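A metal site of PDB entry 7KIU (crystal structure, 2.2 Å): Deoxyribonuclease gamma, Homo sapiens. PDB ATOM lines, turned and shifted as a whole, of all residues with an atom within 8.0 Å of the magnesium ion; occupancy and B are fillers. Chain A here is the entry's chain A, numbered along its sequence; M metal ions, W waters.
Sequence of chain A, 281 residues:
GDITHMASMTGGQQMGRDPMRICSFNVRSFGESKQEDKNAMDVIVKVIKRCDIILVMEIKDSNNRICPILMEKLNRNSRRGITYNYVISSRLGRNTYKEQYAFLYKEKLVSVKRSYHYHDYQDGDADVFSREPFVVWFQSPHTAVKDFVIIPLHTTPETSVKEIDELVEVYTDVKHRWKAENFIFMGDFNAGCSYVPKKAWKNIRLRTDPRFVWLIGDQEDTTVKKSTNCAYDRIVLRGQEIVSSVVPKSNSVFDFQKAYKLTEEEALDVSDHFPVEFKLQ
The side-chain carboxylate (OD2) of Asp 221 lies close to the side-chain amide oxygen (OD1) of Asn 229 (3.4 Å). The backbone NH (N) of Cys 230 lies within hydrogen-bond range of the side-chain carboxylate (OD1) of Asp 221 (3.5 Å).
Within 4 Å of the magnesium ion: Asp 221, Thr 223, Lys 225 and Thr 228. Along chain A the residues within 4 Å of the magnesium ion span positions 221 to 228.
Water W1 is bound to the magnesium ion (2.1 Å). The magnesium ion is bound by water W2 (2.1 Å). The magnesium ion is bound by the backbone carbonyl oxygen (O) of Lys 225 (2.2 Å). The magnesium ion is bound by OD2 of Asp 221 (2.2 Å). O of Thr 223 is bound to the magnesium ion. The backbone carbonyl oxygen (O) of Thr 228 binds the magnesium ion, 2.2 Å away. OG1 of Thr 223 binds the magnesium ion (2.6 Å). The magnesium ion has seven donor atoms within binding distance.
Water W1 bridges the side-chain amide oxygen of Asn 229 and the backbone carbonyl oxygen of Lys 226.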
ATOM      1  N   GLU A 220     -20.990  11.374   7.687  1.00  0.00           N
ATOM      2  CA  GLU A 220     -19.586  10.936   7.638  1.00  0.00           C
ATOM      3  C   GLU A 220     -18.910  11.067   9.006  1.00  0.00           C
ATOM      4  O   GLU A 220     -19.390  11.853   9.821  1.00  0.00           O
ATOM      5  CB  GLU A 220     -18.858  11.677   6.525  1.00  0.00           C
ATOM      6  CG  GLU A 220     -19.514  11.528   5.174  1.00  0.00           C
ATOM      7  CD  GLU A 220     -19.046  10.333   4.354  1.00  0.00           C
ATOM      8  OE1 GLU A 220     -19.683   9.267   4.461  1.00  0.00           O
ATOM      9  OE2 GLU A 220     -18.056  10.478   3.614  1.00  0.00           O
ATOM     10  N   ASP A 221     -17.896  10.249   9.265  1.00  0.00           N
ATOM     11  CA  ASP A 221     -17.105  10.375  10.469  1.00  0.00           C
ATOM     12  C   ASP A 221     -15.758  10.949  10.054  1.00  0.00           C
ATOM     13  O   ASP A 221     -15.013  10.299   9.363  1.00  0.00           O
ATOM     14  CB  ASP A 221     -16.939   9.029  11.229  1.00  0.00           C
ATOM     15  CG  ASP A 221     -16.038   9.161  12.474  1.00  0.00           C
ATOM     16  OD1 ASP A 221     -15.939  10.323  12.956  1.00  0.00           O
ATOM     17  OD2 ASP A 221     -15.406   8.178  12.975  1.00  0.00           O
ATOM     18  N   THR A 222     -15.426  12.162  10.502  1.00  0.00           N
ATOM     19  CA  THR A 222     -14.083  12.717  10.288  1.00  0.00           C
ATOM     20  C   THR A 222     -13.217  12.715  11.555  1.00  0.00           C
ATOM     21  O   THR A 222     -12.112  13.242  11.508  1.00  0.00           O
ATOM     22  CB  THR A 222     -14.097  14.113   9.645  1.00  0.00           C
ATOM     23  OG1 THR A 222     -14.684  15.075  10.548  1.00  0.00           O
ATOM     24  CG2 THR A 222     -14.852  14.088   8.308  1.00  0.00           C
ATOM     25  N   THR A 223     -13.710  12.079  12.638  1.00  0.00           N
ATOM     26  CA  THR A 223     -12.955  11.947  13.874  1.00  0.00           C
ATOM     27  C   THR A 223     -12.212  10.622  14.009  1.00  0.00           C
ATOM     28  O   THR A 223     -12.809   9.538  13.900  1.00  0.00           O
ATOM     29  CB  THR A 223     -13.805  12.212  15.151  1.00  0.00           C
ATOM     30  OG1 THR A 223     -14.634  11.101  15.492  1.00  0.00           O
ATOM     31  CG2 THR A 223     -14.661  13.437  14.988  1.00  0.00           C
ATOM     32  N   VAL A 224     -10.919  10.708  14.326  1.00  0.00           N
ATOM     33  CA  VAL A 224     -10.047   9.551  14.505  1.00  0.00           C
ATOM     34  C   VAL A 224     -10.541   8.708  15.653  1.00  0.00           C
ATOM     35  O   VAL A 224     -10.628   7.502  15.516  1.00  0.00           O
ATOM     36  CB  VAL A 224      -8.594   9.982  14.725  1.00  0.00           C
ATOM     37  CG1 VAL A 224      -7.724   8.792  15.134  1.00  0.00           C
ATOM     38  CG2 VAL A 224      -8.027  10.654  13.488  1.00  0.00           C
ATOM     39  N   LYS A 225     -10.847   9.319  16.797  1.00  0.00           N
ATOM     40  CA  LYS A 225     -11.427   8.559  17.927  1.00  0.00           C
ATOM     41  C   LYS A 225     -12.633   7.712  17.489  1.00  0.00           C
ATOM     42  O   LYS A 225     -13.543   8.192  16.793  1.00  0.00           O
ATOM     43  CB  LYS A 225     -11.895   9.495  19.029  1.00  0.00           C
ATOM     44  CG  LYS A 225     -10.839   9.749  20.066  1.00  0.00           C
ATOM     45  CD  LYS A 225     -11.131  10.912  20.968  1.00  0.00           C
ATOM     46  CE  LYS A 225      -9.888  11.091  21.836  1.00  0.00           C
ATOM     47  NZ  LYS A 225     -10.098  12.095  22.911  1.00  0.00           N
ATOM     48  N   LYS A 226     -12.612   6.458  17.923  1.00  0.00           N
ATOM     49  CA  LYS A 226     -13.698   5.513  17.655  1.00  0.00           C
ATOM     50  C   LYS A 226     -15.014   5.923  18.350  1.00  0.00           C
ATOM     51  O   LYS A 226     -16.063   5.581  17.895  1.00  0.00           O
ATOM     52  CB  LYS A 226     -13.275   4.101  18.079  1.00  0.00           C
ATOM     53  CG  LYS A 226     -14.267   3.006  17.723  1.00  0.00           C
ATOM     54  CD  LYS A 226     -13.987   1.731  18.519  1.00  0.00           C
ATOM     55  CE  LYS A 226     -14.327   0.476  17.740  1.00  0.00           C
ATOM     56  NZ  LYS A 226     -13.561   0.419  16.449  1.00  0.00           N
ATOM     57  N   SER A 227     -14.939   6.636  19.463  1.00  0.00           N
ATOM     58  CA  SER A 227     -16.091   6.918  20.296  1.00  0.00           C
ATOM     59  C   SER A 227     -16.930   8.045  19.716  1.00  0.00           C
ATOM     60  O   SER A 227     -18.048   8.255  20.124  1.00  0.00           O
ATOM     61  CB  SER A 227     -15.675   7.250  21.741  1.00  0.00           C
ATOM     62  OG  SER A 227     -14.787   8.369  21.785  1.00  0.00           O
ATOM     63  N   THR A 228     -16.377   8.780  18.757  1.00  0.00           N
ATOM     64  CA  THR A 228     -17.144   9.837  18.158  1.00  0.00           C
ATOM     65  C   THR A 228     -17.285   9.627  16.669  1.00  0.00           C
ATOM     66  O   THR A 228     -16.374   9.039  16.003  1.00  0.00           O
ATOM     67  CB  THR A 228     -16.549  11.223  18.493  1.00  0.00           C
ATOM     68  OG1 THR A 228     -15.186  11.290  18.041  1.00  0.00           O
ATOM     69  CG2 THR A 228     -16.657  11.453  19.989  1.00  0.00           C
ATOM     70  N   ASN A 229     -18.454  10.072  16.175  1.00  0.00           N
ATOM     71  CA  ASN A 229     -18.864   9.988  14.789  1.00  0.00           C
ATOM     72  C   ASN A 229     -19.467  11.351  14.395  1.00  0.00           C
ATOM     73  O   ASN A 229     -20.655  11.567  14.550  1.00  0.00           O
ATOM     74  CB  ASN A 229     -19.901   8.871  14.616  1.00  0.00           C
ATOM     75  CG  ASN A 229     -19.309   7.486  14.862  1.00  0.00           C
ATOM     76  OD1 ASN A 229     -18.435   7.030  14.099  1.00  0.00           O
ATOM     77  ND2 ASN A 229     -19.720   6.827  15.986  1.00  0.00           N
ATOM     78  N   CYS A 230     -18.603  12.287  14.012  1.00  0.00           N
ATOM     79  CA  CYS A 230     -19.062  13.620  13.564  1.00  0.00           C
ATOM     80  C   CYS A 230     -18.343  14.043  12.276  1.00  0.00           C
ATOM     81  O   CYS A 230     -17.152  13.756  12.169  1.00  0.00           O
ATOM     82  CB  CYS A 230     -18.912  14.733  14.599  1.00  0.00           C
ATOM     83  SG  CYS A 230     -18.873  14.336  16.366  1.00  0.00           S
ATOM     84  N   ASP A 255      -9.373   7.270   5.713  1.00  0.00           N
ATOM     85  CA  ASP A 255      -9.045   6.662   7.028  1.00  0.00           C
ATOM     86  C   ASP A 255      -7.596   6.196   7.042  1.00  0.00           C
ATOM     87  O   ASP A 255      -7.366   5.024   6.705  1.00  0.00           O
ATOM     88  CB  ASP A 255      -9.927   5.432   7.256  1.00  0.00           C
ATOM     89  CG  ASP A 255     -10.093   5.087   8.709  1.00  0.00           C
ATOM     90  OD1 ASP A 255      -9.063   4.952   9.399  1.00  0.00           O
ATOM     91  OD2 ASP A 255     -11.245   4.939   9.143  1.00  0.00           O
ATOM     92  N   GLN A 257      -5.722   5.518   9.459  1.00  0.00           N
ATOM     93  CA  GLN A 257      -5.525   4.513  10.485  1.00  0.00           C
ATOM     94  C   GLN A 257      -5.683   3.099   9.935  1.00  0.00           C
ATOM     95  O   GLN A 257      -4.859   2.245  10.237  1.00  0.00           O
ATOM     96  CB  GLN A 257      -6.494   4.752  11.652  1.00  0.00           C
ATOM     97  CG  GLN A 257      -6.681   3.574  12.579  1.00  0.00           C
ATOM     98  CD  GLN A 257      -7.281   3.986  13.879  1.00  0.00           C
ATOM     99  OE1 GLN A 257      -6.832   3.519  14.941  1.00  0.00           O
ATOM    100  NE2 GLN A 257      -8.272   4.885  13.835  1.00  0.00           N
ATOM    101  N   GLU A 264      -5.014   3.117  17.731  1.00  0.00           N
ATOM    102  CA  GLU A 264      -5.656   4.382  18.046  1.00  0.00           C
ATOM    103  C   GLU A 264      -4.656   5.433  18.556  1.00  0.00           C
ATOM    104  O   GLU A 264      -4.736   6.620  18.146  1.00  0.00           O
ATOM    105  CB  GLU A 264      -6.846   4.217  19.026  1.00  0.00           C
ATOM    106  CG  GLU A 264      -7.908   5.352  18.924  1.00  0.00           C
ATOM    107  CD  GLU A 264      -9.265   5.018  19.610  1.00  0.00           C
ATOM    108  OE1 GLU A 264      -9.417   3.969  20.317  1.00  0.00           O
ATOM    109  OE2 GLU A 264     -10.206   5.809  19.435  1.00  0.00           O
ATOM    110  N   ASP A 272      -6.230  14.292  15.371  1.00  0.00           N
ATOM    111  CA  ASP A 272      -7.549  13.931  15.877  1.00  0.00           C
ATOM    112  C   ASP A 272      -8.600  13.894  14.752  1.00  0.00           C
ATOM    113  O   ASP A 272      -9.703  13.440  14.943  1.00  0.00           O
ATOM    114  CB  ASP A 272      -7.991  14.844  17.054  1.00  0.00           C
ATOM    115  CG  ASP A 272      -7.888  16.345  16.764  1.00  0.00           C
ATOM    116  OD1 ASP A 272      -7.291  16.783  15.753  1.00  0.00           O
ATOM    117  OD2 ASP A 272      -8.405  17.125  17.599  1.00  0.00           O
ATOM    118  N   PHE A 274      -9.421  12.947  10.565  1.00  0.00           N
ATOM    119  CA  PHE A 274      -9.082  12.344   9.302  1.00  0.00           C
ATOM    120  C   PHE A 274      -9.166  13.404   8.198  1.00  0.00           C
ATOM    121  O   PHE A 274      -9.988  14.307   8.248  1.00  0.00           O
ATOM    122  CB  PHE A 274     -10.094  11.294   8.890  1.00  0.00           C
ATOM    123  CG  PHE A 274     -10.058  10.034   9.701  1.00  0.00           C
ATOM    124  CD1 PHE A 274      -8.862   9.375   9.979  1.00  0.00           C
ATOM    125  CD2 PHE A 274     -11.238   9.467  10.174  1.00  0.00           C
ATOM    126  CE1 PHE A 274      -8.854   8.197  10.697  1.00  0.00           C
ATOM    127  CE2 PHE A 274     -11.211   8.271  10.922  1.00  0.00           C
ATOM    128  CZ  PHE A 274     -10.027   7.665  11.160  1.00  0.00           C
HETATM  129 MG    MG M   1     -14.505   8.593  14.900  1.00  0.00          MG
HETATM  130  O   HOH W   1     -15.759   6.966  14.933  1.00  0.00           O
HETATM  131  O   HOH W   2     -13.341   6.977  14.342  1.00  0.00           O
